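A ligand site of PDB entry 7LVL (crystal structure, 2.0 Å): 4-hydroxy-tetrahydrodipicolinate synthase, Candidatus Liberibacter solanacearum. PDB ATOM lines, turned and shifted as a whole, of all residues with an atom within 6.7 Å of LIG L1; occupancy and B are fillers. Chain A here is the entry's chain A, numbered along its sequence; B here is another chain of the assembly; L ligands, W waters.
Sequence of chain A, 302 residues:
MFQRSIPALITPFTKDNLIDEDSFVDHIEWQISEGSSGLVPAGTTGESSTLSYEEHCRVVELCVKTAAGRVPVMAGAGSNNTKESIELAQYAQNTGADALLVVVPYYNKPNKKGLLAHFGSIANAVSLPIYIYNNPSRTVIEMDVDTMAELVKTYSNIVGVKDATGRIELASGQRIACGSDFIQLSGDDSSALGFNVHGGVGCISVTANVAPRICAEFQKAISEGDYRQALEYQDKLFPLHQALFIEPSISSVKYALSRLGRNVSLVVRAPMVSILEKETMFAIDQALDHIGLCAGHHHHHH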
ATOM      1  N   ALA A  42      14.135   3.869  18.117  1.00  0.00           N
ATOM      2  CA  ALA A  42      13.492   4.425  16.915  1.00  0.00           C
ATOM      3  C   ALA A  42      12.021   4.816  17.163  1.00  0.00           C
ATOM      4  O   ALA A  42      11.157   4.590  16.318  1.00  0.00           O
ATOM      5  CB  ALA A  42      13.583   3.447  15.731  1.00  0.00           C
ATOM      6  N   GLU A  47      13.948  10.256  17.216  1.00  0.00           N
ATOM      7  CA  GLU A  47      13.902  11.045  15.971  1.00  0.00           C
ATOM      8  C   GLU A  47      13.540  10.180  14.764  1.00  0.00           C
ATOM      9  O   GLU A  47      14.048  10.387  13.656  1.00  0.00           O
ATOM     10  CB  GLU A  47      15.218  11.779  15.732  1.00  0.00           C
ATOM     11  CG  GLU A  47      15.446  12.918  16.728  1.00  0.00           C
ATOM     12  CD  GLU A  47      16.816  13.588  16.579  1.00  0.00           C
ATOM     13  OE1 GLU A  47      16.944  14.440  15.669  1.00  0.00           O
ATOM     14  OE2 GLU A  47      17.737  13.270  17.375  1.00  0.00           O
ATOM     15  N   SER A  48      12.650   9.205  14.969  1.00  0.00           N
ATOM     16  CA  SER A  48      12.259   8.319  13.878  1.00  0.00           C
ATOM     17  C   SER A  48      11.729   9.093  12.665  1.00  0.00           C
ATOM     18  O   SER A  48      11.877   8.637  11.523  1.00  0.00           O
ATOM     19  CB  SER A  48      11.201   7.305  14.356  1.00  0.00           C
ATOM     20  OG  SER A  48      10.069   7.963  14.912  1.00  0.00           O
ATOM     21  N   SER A  49      11.128  10.270  12.883  1.00  0.00           N
ATOM     22  CA  SER A  49      10.615  11.063  11.760  1.00  0.00           C
ATOM     23  C   SER A  49      11.700  11.458  10.752  1.00  0.00           C
ATOM     24  O   SER A  49      11.410  11.664   9.563  1.00  0.00           O
ATOM     25  CB  SER A  49       9.933  12.326  12.308  1.00  0.00           C
ATOM     26  OG  SER A  49       8.666  12.011  12.871  1.00  0.00           O
ATOM     27  N   THR A  50      12.951  11.581  11.208  1.00  0.00           N
ATOM     28  CA  THR A  50      14.036  12.056  10.360  1.00  0.00           C
ATOM     29  C   THR A  50      15.047  10.961  10.028  1.00  0.00           C
ATOM     30  O   THR A  50      16.119  11.261   9.473  1.00  0.00           O
ATOM     31  CB  THR A  50      14.741  13.241  11.028  1.00  0.00           C
ATOM     32  OG1 THR A  50      15.099  12.886  12.366  1.00  0.00           O
ATOM     33  CG2 THR A  50      13.805  14.451  11.062  1.00  0.00           C
ATOM     34  N   LEU A  51      14.731   9.709  10.345  1.00  0.00           N
ATOM     35  CA  LEU A  51      15.504   8.551   9.890  1.00  0.00           C
ATOM     36  C   LEU A  51      14.981   8.078   8.539  1.00  0.00           C
ATOM     37  O   LEU A  51      13.765   8.058   8.316  1.00  0.00           O
ATOM     38  CB  LEU A  51      15.399   7.407  10.901  1.00  0.00           C
ATOM     39  CG  LEU A  51      15.835   7.670  12.353  1.00  0.00           C
ATOM     40  CD1 LEU A  51      15.676   6.414  13.199  1.00  0.00           C
ATOM     41  CD2 LEU A  51      17.308   8.155  12.418  1.00  0.00           C
ATOM     42  N   SER A  52      15.880   7.642   7.647  1.00  0.00           N
ATOM     43  CA  SER A  52      15.411   6.877   6.496  1.00  0.00           C
ATOM     44  C   SER A  52      14.883   5.520   6.966  1.00  0.00           C
ATOM     45  O   SER A  52      15.060   5.118   8.117  1.00  0.00           O
ATOM     46  CB  SER A  52      16.544   6.649   5.470  1.00  0.00           C
ATOM     47  OG  SER A  52      17.537   5.780   5.990  1.00  0.00           O
ATOM     48  N   TYR A  53      14.215   4.809   6.053  1.00  0.00           N
ATOM     49  CA  TYR A  53      13.822   3.443   6.332  1.00  0.00           C
ATOM     50  C   TYR A  53      15.025   2.620   6.771  1.00  0.00           C
ATOM     51  O   TYR A  53      14.968   1.906   7.781  1.00  0.00           O
ATOM     52  CB  TYR A  53      13.158   2.807   5.103  1.00  0.00           C
ATOM     53  CG  TYR A  53      12.714   1.378   5.335  1.00  0.00           C
ATOM     54  CD1 TYR A  53      11.628   1.081   6.155  1.00  0.00           C
ATOM     55  CD2 TYR A  53      13.406   0.313   4.757  1.00  0.00           C
ATOM     56  CE1 TYR A  53      11.230  -0.229   6.387  1.00  0.00           C
ATOM     57  CE2 TYR A  53      13.005  -1.002   4.973  1.00  0.00           C
ATOM     58  CZ  TYR A  53      11.920  -1.269   5.789  1.00  0.00           C
ATOM     59  OH  TYR A  53      11.523  -2.560   6.009  1.00  0.00           O
ATOM     60  N   HIS A  56      16.306   3.652  10.260  1.00  0.00           N
ATOM     61  CA  HIS A  56      15.354   3.155  11.256  1.00  0.00           C
ATOM     62  C   HIS A  56      15.591   1.672  11.527  1.00  0.00           C
ATOM     63  O   HIS A  56      15.761   1.274  12.684  1.00  0.00           O
ATOM     64  CB  HIS A  56      13.920   3.419  10.754  1.00  0.00           C
ATOM     65  CG  HIS A  56      12.867   3.183  11.800  1.00  0.00           C
ATOM     66  ND1 HIS A  56      11.829   4.063  12.005  1.00  0.00           N
ATOM     67  CD2 HIS A  56      12.670   2.155  12.658  1.00  0.00           C
ATOM     68  CE1 HIS A  56      11.040   3.595  12.964  1.00  0.00           C
ATOM     69  NE2 HIS A  56      11.532   2.433  13.377  1.00  0.00           N
ATOM     70  N   GLY A  78       6.097   3.014  14.138  1.00  0.00           N
ATOM     71  CA  GLY A  78       5.017   3.971  13.924  1.00  0.00           C
ATOM     72  C   GLY A  78       5.134   4.666  12.581  1.00  0.00           C
ATOM     73  O   GLY A  78       6.220   5.046  12.152  1.00  0.00           O
ATOM     74  N   SER A  79       3.996   4.814  11.928  1.00  0.00           N
ATOM     75  CA  SER A  79       3.905   5.572  10.686  1.00  0.00           C
ATOM     76  C   SER A  79       2.464   6.021  10.527  1.00  0.00           C
ATOM     77  O   SER A  79       1.546   5.453  11.130  1.00  0.00           O
ATOM     78  CB  SER A  79       4.362   4.717   9.494  1.00  0.00           C
ATOM     79  OG  SER A  79       4.236   5.410   8.278  1.00  0.00           O
ATOM     80  N   ASN A  80       2.252   7.046   9.710  1.00  0.00           N
ATOM     81  CA  ASN A  80       0.898   7.407   9.312  1.00  0.00           C
ATOM     82  C   ASN A  80       0.496   6.731   8.007  1.00  0.00           C
ATOM     83  O   ASN A  80      -0.570   7.027   7.463  1.00  0.00           O
ATOM     84  CB  ASN A  80       0.770   8.934   9.198  1.00  0.00           C
ATOM     85  CG  ASN A  80       1.727   9.528   8.172  1.00  0.00           C
ATOM     86  OD1 ASN A  80       2.621   8.845   7.684  1.00  0.00           O
ATOM     87  ND2 ASN A  80       1.552  10.794   7.875  1.00  0.00           N
ATOM     88  N   ASN A  81       1.341   5.829   7.519  1.00  0.00           N
ATOM     89  CA  ASN A  81       1.146   5.030   6.319  1.00  0.00           C
ATOM     90  C   ASN A  81       1.150   3.567   6.746  1.00  0.00           C
ATOM     91  O   ASN A  81       2.193   3.034   7.133  1.00  0.00           O
ATOM     92  CB  ASN A  81       2.273   5.320   5.317  1.00  0.00           C
ATOM     93  CG  ASN A  81       2.187   4.486   4.047  1.00  0.00           C
ATOM     94  OD1 ASN A  81       1.328   3.610   3.919  1.00  0.00           O
ATOM     95  ND2 ASN A  81       3.068   4.769   3.091  1.00  0.00           N
ATOM     96  N   GLU A  84       3.912   1.317   5.343  1.00  0.00           N
ATOM     97  CA  GLU A  84       5.230   1.513   5.955  1.00  0.00           C
ATOM     98  C   GLU A  84       5.308   0.886   7.336  1.00  0.00           C
ATOM     99  O   GLU A  84       6.348   0.371   7.725  1.00  0.00           O
ATOM    100  CB  GLU A  84       5.546   3.000   6.087  1.00  0.00           C
ATOM    101  CG  GLU A  84       6.102   3.690   4.858  1.00  0.00           C
ATOM    102  CD  GLU A  84       6.333   5.175   5.128  1.00  0.00           C
ATOM    103  OE1 GLU A  84       7.299   5.480   5.866  1.00  0.00           O
ATOM    104  OE2 GLU A  84       5.537   6.008   4.640  1.00  0.00           O
ATOM    105  N   LEU A  88       8.153  -1.863   8.613  1.00  0.00           N
ATOM    106  CA  LEU A  88       8.960  -1.678   9.823  1.00  0.00           C
ATOM    107  C   LEU A  88       8.660  -2.768  10.858  1.00  0.00           C
ATOM    108  O   LEU A  88       9.558  -3.256  11.550  1.00  0.00           O
ATOM    109  CB  LEU A  88       8.721  -0.298  10.437  1.00  0.00           C
ATOM    110  CG  LEU A  88       9.193   0.948   9.668  1.00  0.00           C
ATOM    111  CD1 LEU A  88       8.571   2.231  10.237  1.00  0.00           C
ATOM    112  CD2 LEU A  88      10.723   1.043   9.674  1.00  0.00           C
ATOM    113  N   TYR A 106      -0.531  10.096  12.503  1.00  0.00           N
ATOM    114  CA  TYR A 106      -0.458  11.548  12.602  1.00  0.00           C
ATOM    115  C   TYR A 106      -0.696  12.194  11.243  1.00  0.00           C
ATOM    116  O   TYR A 106      -0.463  11.579  10.195  1.00  0.00           O
ATOM    117  CB  TYR A 106       0.915  12.002  13.109  1.00  0.00           C
ATOM    118  CG  TYR A 106       2.029  11.176  12.503  1.00  0.00           C
ATOM    119  CD1 TYR A 106       2.638  11.561  11.300  1.00  0.00           C
ATOM    120  CD2 TYR A 106       2.458   9.993  13.110  1.00  0.00           C
ATOM    121  CE1 TYR A 106       3.662  10.782  10.725  1.00  0.00           C
ATOM    122  CE2 TYR A 106       3.475   9.230  12.550  1.00  0.00           C
ATOM    123  CZ  TYR A 106       4.071   9.623  11.359  1.00  0.00           C
ATOM    124  OH  TYR A 106       5.068   8.850  10.800  1.00  0.00           O
ATOM    125  N   SER B  49       0.692  11.522   2.295  1.00  0.00           N
ATOM    126  CA  SER B  49       1.229  10.729   3.396  1.00  0.00           C
ATOM    127  C   SER B  49       1.394   9.256   3.030  1.00  0.00           C
ATOM    128  O   SER B  49       2.253   8.579   3.595  1.00  0.00           O
ATOM    129  CB  SER B  49       0.318  10.834   4.628  1.00  0.00           C
ATOM    130  OG  SER B  49       0.315  12.145   5.124  1.00  0.00           O
ATOM    131  N   SER B  79       6.780  17.751   4.258  1.00  0.00           N
ATOM    132  CA  SER B  79       7.263  16.624   5.052  1.00  0.00           C
ATOM    133  C   SER B  79       7.539  17.167   6.443  1.00  0.00           C
ATOM    134  O   SER B  79       7.682  18.376   6.627  1.00  0.00           O
ATOM    135  CB  SER B  79       8.517  16.010   4.420  1.00  0.00           C
ATOM    136  OG  SER B  79       9.208  15.166   5.314  1.00  0.00           O
ATOM    137  N   ASN B  80       7.592  16.271   7.438  1.00  0.00           N
ATOM    138  CA  ASN B  80       8.133  16.669   8.747  1.00  0.00           C
ATOM    139  C   ASN B  80       9.639  16.436   8.843  1.00  0.00           C
ATOM    140  O   ASN B  80      10.211  16.552   9.936  1.00  0.00           O
ATOM    141  CB  ASN B  80       7.419  15.939   9.893  1.00  0.00           C
ATOM    142  CG  ASN B  80       7.501  14.424   9.779  1.00  0.00           C
ATOM    143  OD1 ASN B  80       8.009  13.876   8.792  1.00  0.00           O
ATOM    144  ND2 ASN B  80       6.985  13.731  10.789  1.00  0.00           N
ATOM    145  N   ASN B  81      10.271  16.100   7.728  1.00  0.00           N
ATOM    146  CA  ASN B  81      11.705  15.817   7.662  1.00  0.00           C
ATOM    147  C   ASN B  81      12.296  16.792   6.654  1.00  0.00           C
ATOM    148  O   ASN B  81      12.027  16.697   5.452  1.00  0.00           O
ATOM    149  CB  ASN B  81      11.921  14.349   7.267  1.00  0.00           C
ATOM    150  CG  ASN B  81      13.396  13.981   7.091  1.00  0.00           C
ATOM    151  OD1 ASN B  81      14.279  14.824   7.170  1.00  0.00           O
ATOM    152  ND2 ASN B  81      13.640  12.685   6.853  1.00  0.00           N
ATOM    153  N   GLU B  84      13.834  15.406   3.509  1.00  0.00           N
ATOM    154  CA  GLU B  84      12.852  14.938   2.535  1.00  0.00           C
ATOM    155  C   GLU B  84      12.184  16.095   1.794  1.00  0.00           C
ATOM    156  O   GLU B  84      11.915  16.000   0.593  1.00  0.00           O
ATOM    157  CB  GLU B  84      11.763  14.096   3.206  1.00  0.00           C
ATOM    158  CG  GLU B  84      12.165  12.708   3.695  1.00  0.00           C
ATOM    159  CD  GLU B  84      10.983  11.975   4.368  1.00  0.00           C
ATOM    160  OE1 GLU B  84       9.943  11.783   3.683  1.00  0.00           O
ATOM    161  OE2 GLU B  84      11.092  11.604   5.570  1.00  0.00           O
ATOM    162  N   TYR B 106       4.647  18.291  10.846  1.00  0.00           N
ATOM    163  CA  TYR B 106       3.680  17.616  11.702  1.00  0.00           C
ATOM    164  C   TYR B 106       4.374  16.580  12.586  1.00  0.00           C
ATOM    165  O   TYR B 106       5.476  16.113  12.278  1.00  0.00           O
ATOM    166  CB  TYR B 106       2.606  16.917  10.856  1.00  0.00           C
ATOM    167  CG  TYR B 106       3.208  16.240   9.634  1.00  0.00           C
ATOM    168  CD1 TYR B 106       3.662  14.928   9.696  1.00  0.00           C
ATOM    169  CD2 TYR B 106       3.350  16.927   8.423  1.00  0.00           C
ATOM    170  CE1 TYR B 106       4.229  14.300   8.581  1.00  0.00           C
ATOM    171  CE2 TYR B 106       3.910  16.312   7.294  1.00  0.00           C
ATOM    172  CZ  TYR B 106       4.356  15.007   7.391  1.00  0.00           C
ATOM    173  OH  TYR B 106       4.923  14.390   6.285  1.00  0.00           O
ATOM    174  N   TYR B 107       3.704  16.230  13.679  1.00  0.00           N
ATOM    175  CA  TYR B 107       4.060  15.160  14.606  1.00  0.00           C
ATOM    176  C   TYR B 107       5.264  15.483  15.499  1.00  0.00           C
ATOM    177  O   TYR B 107       5.143  15.367  16.727  1.00  0.00           O
ATOM    178  CB  TYR B 107       4.301  13.831  13.873  1.00  0.00           C
ATOM    179  CG  TYR B 107       4.491  12.705  14.870  1.00  0.00           C
ATOM    180  CD1 TYR B 107       3.437  12.280  15.667  1.00  0.00           C
ATOM    181  CD2 TYR B 107       5.730  12.115  15.070  1.00  0.00           C
ATOM    182  CE1 TYR B 107       3.589  11.283  16.597  1.00  0.00           C
ATOM    183  CE2 TYR B 107       5.905  11.110  15.997  1.00  0.00           C
ATOM    184  CZ  TYR B 107       4.834  10.714  16.770  1.00  0.00           C
ATOM    185  OH  TYR B 107       4.982   9.715  17.713  1.00  0.00           O
ATOM    186  N   ASN B 108       6.411  15.890  14.936  1.00  0.00           N
ATOM    187  CA  ASN B 108       7.596  16.110  15.764  1.00  0.00           C
ATOM    188  C   ASN B 108       7.664  17.514  16.391  1.00  0.00           C
ATOM    189  O   ASN B 108       8.550  17.758  17.216  1.00  0.00           O
ATOM    190  CB  ASN B 108       8.894  15.779  14.997  1.00  0.00           C
ATOM    191  CG  ASN B 108       9.036  16.507  13.657  1.00  0.00           C
ATOM    192  OD1 ASN B 108       8.243  17.391  13.318  1.00  0.00           O
ATOM    193  ND2 ASN B 108      10.069  16.156  12.905  1.00  0.00           N
HETATM  194  N1  LIG L   1       9.359  11.463   7.981  1.00  0.00           N
HETATM  195  C1  LIG L   1       8.422  10.396   7.618  1.00  0.00           C
HETATM  196  C2  LIG L   1       7.413  10.183   8.747  1.00  0.00           C
HETATM  197  O1  LIG L   1       7.573  10.773   9.856  1.00  0.00           O
HETATM  198  C3  LIG L   1       9.181   9.097   7.280  1.00  0.00           C
HETATM  199  C4  LIG L   1       9.945   8.434   8.444  1.00  0.00           C
HETATM  200  C5  LIG L   1      10.315   7.005   8.011  1.00  0.00           C
HETATM  201  C6  LIG L   1      11.229   6.264   9.001  1.00  0.00           C
HETATM  202  N2  LIG L   1      10.708   6.290  10.359  1.00  0.00           N
HETATM  203  O2  LIG L   1       6.397   9.439   8.582  1.00  0.00           O
HETATM  204  N1  LG2 L   2       4.273   8.796   5.349  1.00  0.00           N
HETATM  205  C1  LG2 L   2       5.419   9.676   5.482  1.00  0.00           C
HETATM  206  C2  LG2 L   2       4.915  11.085   5.828  1.00  0.00           C
HETATM  207  O1  LG2 L   2       5.723  11.992   6.176  1.00  0.00           O
HETATM  208  C3  LG2 L   2       6.279   9.662   4.195  1.00  0.00           C
HETATM  209  C4  LG2 L   2       5.593  10.239   2.946  1.00  0.00           C
HETATM  210  C5  LG2 L   2       6.695  10.540   1.909  1.00  0.00           C
HETATM  211  C6  LG2 L   2       6.138  10.748   0.484  1.00  0.00           C
HETATM  212  N2  LG2 L   2       5.187  11.846   0.432  1.00  0.00           N
HETATM  213  O2  LG2 L   2       3.675  11.317   5.766  1.00  0.00           O
HETATM  214  O   HOH W   1       7.446   9.800  12.402  1.00  0.00           O
HETATM  215  O   HOH W   2       7.999   5.616   9.953  1.00  0.00           O
HETATM  216  O   HOH W   3       6.325   6.871   8.026  1.00  0.00           O
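Water W3 lies within hydrogen-bond range of the side-chain hydroxyl of Ser 79 of chain A (2.6 Å), an oxygen (O2) of LIG L1 (2.6 Å) and the side-chain carboxylate of Glu 84 of chain A (2.7 Å).
Water W1 lies within hydrogen-bond range of the side-chain hydroxyl of Ser 49 of chain A (2.6 Å), an oxygen (O1) of LIG L1 (2.7 Å) and the side-chain hydroxyl of Tyr 106 of chain A (3.0 Å).
Water W2 bridges N2 of LIG L1 and O of Gly 78.
The backbone carbonyl oxygen of Tyr 106 of chain A lies close to the side-chain amide nitrogen of Asn 80 of chain A (3.2 Å).
The side-chain hydroxyl (OG) of Ser 49 of chain A sits at hydrogen-bond distance from the side-chain amide nitrogen (ND2) of Asn 80 of chain B, at 3.2 Å.
The side-chain amide nitrogen (ND2) of Asn 108 of chain B sits at hydrogen-bond distance from the backbone carbonyl oxygen (O) of Asn 80 of chain B (3.0 Å).
The side-chain amide nitrogen (ND2) of Asn 80 of chain A lies within hydrogen-bond range of the side-chain hydroxyl (OG) of Ser 49 of chain B (3.3 Å).
OG of Ser 79 of chain B sits at hydrogen-bond distance from N of Asn 81 of chain B, at 2.8 Å.
The side-chain carboxylate (OE2) of Glu 84 of chain B is in hydrogen-bond range of the side-chain amide nitrogen (ND2) of Asn 81 of chain B (3.1 Å).
The side-chain amide nitrogen (ND2) of Asn 80 of chain B lies close to the backbone carbonyl oxygen (O) of Tyr 106 of chain B (3.2 Å).
Residues that only touch LIG L1: Leu 51, Asn 81 of chain B and Asn 80 of chain A.
Hydrophobic or aromatic side chains within 4 Å of LIG L1: His 56 and Tyr 106 of chain A.
Nine residues have an atom within 4 Å of LIG L1: Ser 48, Ser 49 of chain A, Leu 51, His 56, Asn 80 of chain A, Tyr 106 of chain A, Asn 80 of chain B, Asn 81 of chain B and Glu 84 of chain B.
The nearest printed residue that does not touch LIG L1 is Glu 84 of chain A (4.003 Å).
OD1 of Asn 80 of chain A is in hydrogen-bond range of N1 of LG2 L2, at 2.9 Å.
The side-chain hydroxyl (OG) of Ser 49 of chain A lies within hydrogen-bond range of an oxygen (O1) of LIG L1 (3.4 Å).
The backbone carbonyl oxygen (O) of Ser 48 is in hydrogen-bond range of a nitrogen (N2) of LIG L1, at 2.9 Å.
The side-chain carboxylate (OE2) of Glu 84 of chain A lies within salt-bridge range of a nitrogen (N1) of LG2 L2.
A nitrogen (N1) of LG2 L2 lies within hydrogen-bond range of the backbone carbonyl oxygen (O) of Ser 49 of chain B.
A nitrogen (N1) of LIG L1 sits at hydrogen-bond distance from the side-chain amide oxygen (OD1) of Asn 80 of chain B (2.9 Å).
The side-chain carboxylate (OE2) of Glu 84 of chain B lies within salt-bridge range of a nitrogen (N1) of LIG L1 (3.0 Å).
O1 of LG2 L2 lies within hydrogen-bond range of OH of Tyr 106 of chain B (2.5 Å).
A nitrogen (N1) of LIG L1 is in hydrogen-bond range of the backbone carbonyl oxygen (O) of Ser 49 of chain A, 2.6 Å away.
A ring nitrogen (ND1) of His 56 sits at hydrogen-bond distance from a nitrogen (N2) of LIG L1, at 3.0 Å.
The side-chain hydroxyl (OH) of Tyr 106 of chain A lies within hydrogen-bond range of an oxygen (O2) of LIG L1 (2.7 Å).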
